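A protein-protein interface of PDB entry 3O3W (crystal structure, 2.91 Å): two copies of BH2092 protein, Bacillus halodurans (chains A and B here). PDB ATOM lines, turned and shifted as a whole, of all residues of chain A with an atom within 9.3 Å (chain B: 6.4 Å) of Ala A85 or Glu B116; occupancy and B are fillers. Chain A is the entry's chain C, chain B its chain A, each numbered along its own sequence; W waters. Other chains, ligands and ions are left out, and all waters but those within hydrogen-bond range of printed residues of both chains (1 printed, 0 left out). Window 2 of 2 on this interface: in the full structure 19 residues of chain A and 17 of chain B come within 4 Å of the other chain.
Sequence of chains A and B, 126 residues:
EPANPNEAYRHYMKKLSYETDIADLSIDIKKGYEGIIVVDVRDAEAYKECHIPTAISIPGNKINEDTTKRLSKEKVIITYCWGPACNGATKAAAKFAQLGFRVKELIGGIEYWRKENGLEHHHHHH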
ATOM      1  N   CYS A  81      12.131 -32.164  -5.434  1.00  0.00           N
ATOM      2  CA  CYS A  81      13.232 -31.233  -5.271  1.00  0.00           C
ATOM      3  C   CYS A  81      13.757 -31.334  -3.835  1.00  0.00           C
ATOM      4  O   CYS A  81      13.663 -32.389  -3.218  1.00  0.00           O
ATOM      5  CB  CYS A  81      12.768 -29.787  -5.607  1.00  0.00           C
ATOM      6  SG  CYS A  81      14.077 -28.476  -5.492  1.00  0.00           S
ATOM      7  N   TRP A  82      14.298 -30.239  -3.314  1.00  0.00           N
ATOM      8  CA  TRP A  82      14.833 -30.202  -1.970  1.00  0.00           C
ATOM      9  C   TRP A  82      13.792 -30.239  -0.861  1.00  0.00           C
ATOM     10  O   TRP A  82      13.814 -31.123  -0.019  1.00  0.00           O
ATOM     11  CB  TRP A  82      15.697 -28.963  -1.785  1.00  0.00           C
ATOM     12  CG  TRP A  82      16.942 -28.983  -2.557  1.00  0.00           C
ATOM     13  CD1 TRP A  82      17.159 -28.419  -3.776  1.00  0.00           C
ATOM     14  CD2 TRP A  82      18.166 -29.602  -2.174  1.00  0.00           C
ATOM     15  NE1 TRP A  82      18.460 -28.643  -4.184  1.00  0.00           N
ATOM     16  CE2 TRP A  82      19.098 -29.368  -3.213  1.00  0.00           C
ATOM     17  CE3 TRP A  82      18.575 -30.329  -1.046  1.00  0.00           C
ATOM     18  CZ2 TRP A  82      20.414 -29.849  -3.163  1.00  0.00           C
ATOM     19  CZ3 TRP A  82      19.890 -30.809  -0.996  1.00  0.00           C
ATOM     20  CH2 TRP A  82      20.788 -30.563  -2.048  1.00  0.00           C
ATOM     21  N   GLY A  83      12.889 -29.268  -0.850  1.00  0.00           N
ATOM     22  CA  GLY A  83      11.878 -29.218   0.193  1.00  0.00           C
ATOM     23  C   GLY A  83      10.694 -28.327  -0.143  1.00  0.00           C
ATOM     24  O   GLY A  83      10.539 -27.946  -1.300  1.00  0.00           O
ATOM     25  N   PRO A  84       9.849 -27.973   0.839  1.00  0.00           N
ATOM     26  CA  PRO A  84       8.668 -27.125   0.649  1.00  0.00           C
ATOM     27  C   PRO A  84       8.958 -25.746   0.057  1.00  0.00           C
ATOM     28  O   PRO A  84       8.107 -25.153  -0.597  1.00  0.00           O
ATOM     29  CB  PRO A  84       8.094 -27.026   2.058  1.00  0.00           C
ATOM     30  CG  PRO A  84       8.512 -28.289   2.682  1.00  0.00           C
ATOM     31  CD  PRO A  84       9.936 -28.422   2.238  1.00  0.00           C
ATOM     32  N   ALA A  85      10.159 -25.241   0.292  1.00  0.00           N
ATOM     33  CA  ALA A  85      10.511 -23.925  -0.202  1.00  0.00           C
ATOM     34  C   ALA A  85      10.973 -23.958  -1.648  1.00  0.00           C
ATOM     35  O   ALA A  85      11.273 -22.909  -2.223  1.00  0.00           O
ATOM     36  CB  ALA A  85      11.595 -23.300   0.682  1.00  0.00           C
ATOM     37  N   CYS A  86      11.032 -25.141  -2.253  1.00  0.00           N
ATOM     38  CA  CYS A  86      11.492 -25.227  -3.642  1.00  0.00           C
ATOM     39  C   CYS A  86      10.335 -25.394  -4.629  1.00  0.00           C
ATOM     40  O   CYS A  86       9.273 -25.860  -4.245  1.00  0.00           O
ATOM     41  CB  CYS A  86      12.523 -26.373  -3.793  1.00  0.00           C
ATOM     42  SG  CYS A  86      13.075 -26.680  -5.522  1.00  0.00           S
ATOM     43  N   ASN A  87      10.543 -24.990  -5.884  1.00  0.00           N
ATOM     44  CA  ASN A  87       9.541 -25.096  -6.955  1.00  0.00           C
ATOM     45  C   ASN A  87       9.879 -26.195  -7.945  1.00  0.00           C
ATOM     46  O   ASN A  87       9.040 -26.612  -8.739  1.00  0.00           O
ATOM     47  CB  ASN A  87       9.477 -23.797  -7.743  1.00  0.00           C
ATOM     48  CG  ASN A  87       8.477 -22.848  -7.195  1.00  0.00           C
ATOM     49  OD1 ASN A  87       8.332 -21.725  -7.694  1.00  0.00           O
ATOM     50  ND2 ASN A  87       7.760 -23.280  -6.160  1.00  0.00           N
ATOM     51  N   GLY A  88      11.137 -26.617  -7.899  1.00  0.00           N
ATOM     52  CA  GLY A  88      11.651 -27.634  -8.784  1.00  0.00           C
ATOM     53  C   GLY A  88      10.664 -28.706  -9.153  1.00  0.00           C
ATOM     54  O   GLY A  88      10.398 -28.920 -10.335  1.00  0.00           O
ATOM     55  N   ALA A  89      10.120 -29.382  -8.146  1.00  0.00           N
ATOM     56  CA  ALA A  89       9.166 -30.461  -8.384  1.00  0.00           C
ATOM     57  C   ALA A  89       7.958 -30.006  -9.213  1.00  0.00           C
ATOM     58  O   ALA A  89       7.570 -30.699 -10.163  1.00  0.00           O
ATOM     59  CB  ALA A  89       8.711 -31.055  -7.064  1.00  0.00           C
ATOM     60  N   THR A  90       7.375 -28.859  -8.863  1.00  0.00           N
ATOM     61  CA  THR A  90       6.230 -28.334  -9.592  1.00  0.00           C
ATOM     62  C   THR A  90       6.606 -27.914 -11.012  1.00  0.00           C
ATOM     63  O   THR A  90       5.930 -28.273 -11.984  1.00  0.00           O
ATOM     64  CB  THR A  90       5.625 -27.122  -8.875  1.00  0.00           C
ATOM     65  OG1 THR A  90       5.225 -27.490  -7.548  1.00  0.00           O
ATOM     66  CG2 THR A  90       4.400 -26.610  -9.633  1.00  0.00           C
ATOM     67  N   LYS A  91       7.689 -27.156 -11.134  1.00  0.00           N
ATOM     68  CA  LYS A  91       8.147 -26.713 -12.444  1.00  0.00           C
ATOM     69  C   LYS A  91       8.402 -27.933 -13.316  1.00  0.00           C
ATOM     70  O   LYS A  91       7.859 -28.036 -14.415  1.00  0.00           O
ATOM     71  CB  LYS A  91       9.433 -25.895 -12.313  1.00  0.00           C
ATOM     72  CG  LYS A  91       9.236 -24.517 -11.703  1.00  0.00           C
ATOM     73  CD  LYS A  91      10.538 -23.735 -11.646  1.00  0.00           C
ATOM     74  CE  LYS A  91      10.347 -22.371 -11.008  1.00  0.00           C
ATOM     75  NZ  LYS A  91      11.629 -21.597 -10.933  1.00  0.00           N
ATOM     76  N   ILE A 107       5.326 -33.802  -2.786  1.00  0.00           N
ATOM     77  CA  ILE A 107       5.328 -32.683  -1.859  1.00  0.00           C
ATOM     78  C   ILE A 107       6.230 -33.000  -0.681  1.00  0.00           C
ATOM     79  O   ILE A 107       6.089 -34.049  -0.052  1.00  0.00           O
ATOM     80  CB  ILE A 107       3.914 -32.371  -1.369  1.00  0.00           C
ATOM     81  CG1 ILE A 107       3.283 -33.649  -0.833  1.00  0.00           C
ATOM     82  CG2 ILE A 107       3.081 -31.758  -2.526  1.00  0.00           C
ATOM     83  CD1 ILE A 107       1.840 -33.504  -0.318  1.00  0.00           C
ATOM     84  N   GLY A 108       7.180 -32.098  -0.416  1.00  0.00           N
ATOM     85  CA  GLY A 108       8.106 -32.263   0.693  1.00  0.00           C
ATOM     86  C   GLY A 108       9.552 -32.396   0.276  1.00  0.00           C
ATOM     87  O   GLY A 108      10.438 -31.873   0.946  1.00  0.00           O
ATOM     88  N   GLY A 109       9.787 -33.114  -0.823  1.00  0.00           N
ATOM     89  CA  GLY A 109      11.139 -33.314  -1.324  1.00  0.00           C
ATOM     90  C   GLY A 109      12.040 -34.129  -0.410  1.00  0.00           C
ATOM     91  O   GLY A 109      11.572 -34.839   0.476  1.00  0.00           O
ATOM     92  N   GLU A 111      13.891 -33.213   1.997  1.00  0.00           N
ATOM     93  CA  GLU A 111      13.738 -32.795   3.382  1.00  0.00           C
ATOM     94  C   GLU A 111      12.744 -33.663   4.166  1.00  0.00           C
ATOM     95  O   GLU A 111      13.064 -34.153   5.252  1.00  0.00           O
ATOM     96  CB  GLU A 111      13.307 -31.327   3.420  1.00  0.00           C
ATOM     97  CG  GLU A 111      13.444 -30.669   4.784  1.00  0.00           C
ATOM     98  CD  GLU A 111      13.069 -29.193   4.761  1.00  0.00           C
ATOM     99  OE1 GLU A 111      11.852 -28.874   4.689  1.00  0.00           O
ATOM    100  OE2 GLU A 111      13.996 -28.342   4.807  1.00  0.00           O
ATOM    101  N   TYR A 112      11.544 -33.848   3.618  1.00  0.00           N
ATOM    102  CA  TYR A 112      10.523 -34.660   4.280  1.00  0.00           C
ATOM    103  C   TYR A 112      10.892 -36.141   4.238  1.00  0.00           C
ATOM    104  O   TYR A 112      10.661 -36.890   5.197  1.00  0.00           O
ATOM    105  CB  TYR A 112       9.162 -34.452   3.620  1.00  0.00           C
ATOM    106  CG  TYR A 112       8.492 -33.130   3.949  1.00  0.00           C
ATOM    107  CD1 TYR A 112       9.187 -32.094   4.586  1.00  0.00           C
ATOM    108  CD2 TYR A 112       7.152 -32.913   3.612  1.00  0.00           C
ATOM    109  CE1 TYR A 112       8.563 -30.895   4.876  1.00  0.00           C
ATOM    110  CE2 TYR A 112       6.525 -31.712   3.890  1.00  0.00           C
ATOM    111  CZ  TYR A 112       7.229 -30.705   4.527  1.00  0.00           C
ATOM    112  OH  TYR A 112       6.570 -29.525   4.830  1.00  0.00           O
ATOM    113  N   ASP B  21       8.224 -18.931  -4.860  1.00  0.00           N
ATOM    114  CA  ASP B  21       9.033 -19.488  -3.788  1.00  0.00           C
ATOM    115  C   ASP B  21      10.143 -18.554  -3.364  1.00  0.00           C
ATOM    116  O   ASP B  21      10.328 -17.505  -3.962  1.00  0.00           O
ATOM    117  CB  ASP B  21       9.595 -20.849  -4.202  1.00  0.00           C
ATOM    118  CG  ASP B  21      10.526 -20.755  -5.366  1.00  0.00           C
ATOM    119  OD1 ASP B  21      10.365 -19.799  -6.153  1.00  0.00           O
ATOM    120  OD2 ASP B  21      11.406 -21.634  -5.506  1.00  0.00           O
ATOM    121  N   ILE B  22      10.871 -18.943  -2.321  1.00  0.00           N
ATOM    122  CA  ILE B  22      11.971 -18.139  -1.788  1.00  0.00           C
ATOM    123  C   ILE B  22      13.072 -17.863  -2.802  1.00  0.00           C
ATOM    124  O   ILE B  22      13.557 -16.745  -2.911  1.00  0.00           O
ATOM    125  CB  ILE B  22      12.637 -18.812  -0.577  1.00  0.00           C
ATOM    126  CG1 ILE B  22      11.589 -19.166   0.466  1.00  0.00           C
ATOM    127  CG2 ILE B  22      13.641 -17.867   0.034  1.00  0.00           C
ATOM    128  CD1 ILE B  22      10.860 -17.974   1.020  1.00  0.00           C
ATOM    129  N   ALA B  23      13.473 -18.889  -3.534  1.00  0.00           N
ATOM    130  CA  ALA B  23      14.520 -18.741  -4.523  1.00  0.00           C
ATOM    131  C   ALA B  23      14.212 -17.675  -5.564  1.00  0.00           C
ATOM    132  O   ALA B  23      14.981 -16.730  -5.732  1.00  0.00           O
ATOM    133  CB  ALA B  23      14.768 -20.062  -5.201  1.00  0.00           C
ATOM    134  N   ILE B 107       4.496 -18.614  -0.875  1.00  0.00           N
ATOM    135  CA  ILE B 107       4.307 -19.789  -0.038  1.00  0.00           C
ATOM    136  C   ILE B 107       5.514 -19.960   0.881  1.00  0.00           C
ATOM    137  O   ILE B 107       6.662 -19.960   0.425  1.00  0.00           O
ATOM    138  CB  ILE B 107       4.093 -21.060  -0.899  1.00  0.00           C
ATOM    139  CG1 ILE B 107       5.220 -21.168  -1.928  1.00  0.00           C
ATOM    140  CG2 ILE B 107       2.703 -21.001  -1.561  1.00  0.00           C
ATOM    141  CD1 ILE B 107       5.161 -22.378  -2.826  1.00  0.00           C
ATOM    142  N   GLU B 111       9.164 -17.556   7.711  1.00  0.00           N
ATOM    143  CA  GLU B 111       9.748 -18.807   8.187  1.00  0.00           C
ATOM    144  C   GLU B 111      10.673 -19.455   7.152  1.00  0.00           C
ATOM    145  O   GLU B 111      11.833 -19.730   7.439  1.00  0.00           O
ATOM    146  CB  GLU B 111       8.632 -19.783   8.576  1.00  0.00           C
ATOM    147  CG  GLU B 111       9.100 -20.961   9.406  1.00  0.00           C
ATOM    148  CD  GLU B 111       7.952 -21.851   9.869  1.00  0.00           C
ATOM    149  OE1 GLU B 111       7.408 -22.610   9.035  1.00  0.00           O
ATOM    150  OE2 GLU B 111       7.578 -21.789  11.067  1.00  0.00           O
ATOM    151  N   TYR B 112      10.166 -19.689   5.947  1.00  0.00           N
ATOM    152  CA  TYR B 112      10.974 -20.301   4.895  1.00  0.00           C
ATOM    153  C   TYR B 112      12.097 -19.359   4.430  1.00  0.00           C
ATOM    154  O   TYR B 112      13.222 -19.783   4.144  1.00  0.00           O
ATOM    155  CB  TYR B 112      10.083 -20.691   3.706  1.00  0.00           C
ATOM    156  CG  TYR B 112       9.213 -21.906   3.929  1.00  0.00           C
ATOM    157  CD1 TYR B 112       9.040 -22.449   5.204  1.00  0.00           C
ATOM    158  CD2 TYR B 112       8.566 -22.516   2.857  1.00  0.00           C
ATOM    159  CE1 TYR B 112       8.245 -23.577   5.402  1.00  0.00           C
ATOM    160  CE2 TYR B 112       7.769 -23.644   3.038  1.00  0.00           C
ATOM    161  CZ  TYR B 112       7.614 -24.175   4.301  1.00  0.00           C
ATOM    162  OH  TYR B 112       6.868 -25.325   4.456  1.00  0.00           O
ATOM    163  N   TRP B 113      11.780 -18.076   4.356  1.00  0.00           N
ATOM    164  CA  TRP B 113      12.763 -17.095   3.943  1.00  0.00           C
ATOM    165  C   TRP B 113      13.974 -17.086   4.887  1.00  0.00           C
ATOM    166  O   TRP B 113      15.114 -17.080   4.421  1.00  0.00           O
ATOM    167  CB  TRP B 113      12.120 -15.713   3.869  1.00  0.00           C
ATOM    168  CG  TRP B 113      13.097 -14.638   3.531  1.00  0.00           C
ATOM    169  CD1 TRP B 113      13.879 -13.936   4.407  1.00  0.00           C
ATOM    170  CD2 TRP B 113      13.451 -14.181   2.215  1.00  0.00           C
ATOM    171  NE1 TRP B 113      14.695 -13.080   3.718  1.00  0.00           N
ATOM    172  CE2 TRP B 113      14.462 -13.210   2.372  1.00  0.00           C
ATOM    173  CE3 TRP B 113      13.024 -14.513   0.920  1.00  0.00           C
ATOM    174  CZ2 TRP B 113      15.047 -12.545   1.287  1.00  0.00           C
ATOM    175  CZ3 TRP B 113      13.604 -13.859  -0.164  1.00  0.00           C
ATOM    176  CH2 TRP B 113      14.615 -12.886   0.027  1.00  0.00           C
ATOM    177  N   ARG B 114      13.742 -17.100   6.200  1.00  0.00           N
ATOM    178  CA  ARG B 114      14.857 -17.120   7.158  1.00  0.00           C
ATOM    179  C   ARG B 114      15.816 -18.263   6.882  1.00  0.00           C
ATOM    180  O   ARG B 114      17.023 -18.060   6.803  1.00  0.00           O
ATOM    181  CB  ARG B 114      14.378 -17.272   8.608  1.00  0.00           C
ATOM    182  CG  ARG B 114      13.713 -16.049   9.201  1.00  0.00           C
ATOM    183  CD  ARG B 114      13.502 -16.186  10.716  1.00  0.00           C
ATOM    184  NE  ARG B 114      12.817 -17.430  11.063  1.00  0.00           N
ATOM    185  CZ  ARG B 114      13.429 -18.564  11.388  1.00  0.00           C
ATOM    186  NH1 ARG B 114      14.750 -18.611  11.423  1.00  0.00           N
ATOM    187  NH2 ARG B 114      12.722 -19.655  11.658  1.00  0.00           N
ATOM    188  N   LYS B 115      15.274 -19.467   6.741  1.00  0.00           N
ATOM    189  CA  LYS B 115      16.092 -20.639   6.506  1.00  0.00           C
ATOM    190  C   LYS B 115      17.038 -20.507   5.325  1.00  0.00           C
ATOM    191  O   LYS B 115      18.144 -21.063   5.347  1.00  0.00           O
ATOM    192  CB  LYS B 115      15.193 -21.855   6.340  1.00  0.00           C
ATOM    193  CG  LYS B 115      14.392 -22.163   7.611  1.00  0.00           C
ATOM    194  CD  LYS B 115      13.385 -23.295   7.420  1.00  0.00           C
ATOM    195  CE  LYS B 115      12.558 -23.511   8.688  1.00  0.00           C
ATOM    196  NZ  LYS B 115      11.398 -24.433   8.486  1.00  0.00           N
ATOM    197  N   GLU B 116      16.629 -19.750   4.311  1.00  0.00           N
ATOM    198  CA  GLU B 116      17.466 -19.567   3.127  1.00  0.00           C
ATOM    199  C   GLU B 116      18.523 -18.454   3.233  1.00  0.00           C
ATOM    200  O   GLU B 116      19.702 -18.717   3.111  1.00  0.00           O
ATOM    201  CB  GLU B 116      16.585 -19.327   1.902  1.00  0.00           C
ATOM    202  CG  GLU B 116      15.302 -20.186   1.858  1.00  0.00           C
ATOM    203  CD  GLU B 116      15.538 -21.681   1.594  1.00  0.00           C
ATOM    204  OE1 GLU B 116      16.087 -22.369   2.489  1.00  0.00           O
ATOM    205  OE2 GLU B 116      15.168 -22.165   0.492  1.00  0.00           O
ATOM    206  N   ASN B 117      18.170 -17.210   3.477  1.00  0.00           N
ATOM    207  CA  ASN B 117      19.255 -16.234   3.540  1.00  0.00           C
ATOM    208  C   ASN B 117      20.166 -16.330   4.826  1.00  0.00           C
ATOM    209  O   ASN B 117      21.013 -15.451   5.111  1.00  0.00           O
ATOM    210  CB  ASN B 117      18.634 -14.867   3.271  1.00  0.00           C
ATOM    211  CG  ASN B 117      18.023 -14.798   1.862  1.00  0.00           C
ATOM    212  OD1 ASN B 117      17.080 -15.531   1.534  1.00  0.00           O
ATOM    213  ND2 ASN B 117      18.578 -13.923   1.019  1.00  0.00           N
ATOM    214  N   GLY B 118      20.025 -17.465   5.534  1.00  0.00           N
ATOM    215  CA  GLY B 118      20.771 -17.740   6.757  1.00  0.00           C
ATOM    216  C   GLY B 118      20.742 -19.196   7.234  1.00  0.00           C
ATOM    217  O   GLY B 118      20.562 -20.106   6.385  1.00  0.00           O
HETATM  218  O   HOH W   1       8.322 -18.619  -7.647  1.00  0.00           O
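OD1 of Asp B21 lies close to OD1 of Asn A87 (3.2 Å).
The side-chain sulfur (SG) of Cys A86 forms a disulfide with the side-chain sulfur (SG) of Cys A81.
Among the printed residues, pairs that only touch across the chains: Pro A84 with Tyr B112 (3.2 Å), Ala A85 with Asp B21 (3.3 Å), Ala A85 with Ile B22 (3.99 Å), Ala A85 with Tyr B112 (3.8 Å) and Ala A85 with Glu B116 (3.8 Å).
Of the printed residues of chain B, Ala A85 touches Asp B21, Ile B22, Tyr B112 and Glu B116. Of chain A, only Ala A85 (3.8 Å) comes within 4 Å of Glu B116. No residue of chain A comes within 4 Å of Gly B118. Of the printed residues of chain B, Pro A84 touches Tyr B112 (3.2 Å). Of the printed residues of chain A, Tyr B112 touches Pro A84 (3.2 Å) and Ala A85 (3.8 Å). Printed residues of chain A within 4 Å of Asp B21: Ala A85 and Asn A87. Printed residues of chain A within 4 Å of Ile B22: Ala A85 (3.99 Å). Printed residues of chain B within 4 Å of Asn A87: Asp B21 (3.2 Å). Ala B23 touches none of the printed residues of chain A. Gly A83 touches none of the printed residues of chain B. The nearest printed residue of chain A that does not touch Tyr B112 is Tyr A112 (4.2 Å).
Of the 16 printed residues of chain A, 3 touch a printed residue of chain B. Hydrophobic or aromatic side chains of chain A that line the printed part of chain B: Pro A84 and Ala A85. Of the 12 printed residues of chain B, 4 touch a printed residue of chain A. Along chain B the printed residues that touch a printed residue of chain A span positions 21 to 116. Among the printed residues, 6 pairs touch across the chains. Among the printed residues, no Asp or Glu carboxylate lies within 4 Å of a Lys or Arg side-chain nitrogen of the other chain.
Positions printed for both chains: 107, 111 and 112. Of the 6 pairs that touch across the chains among the printed residues, none has its exchanged pair printed and touching as well.
Water W1 lies within hydrogen-bond range of the side-chain carboxylate of Asp B21 (2.8 Å) and the side-chain amide oxygen of Asn A87 (3.1 Å).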
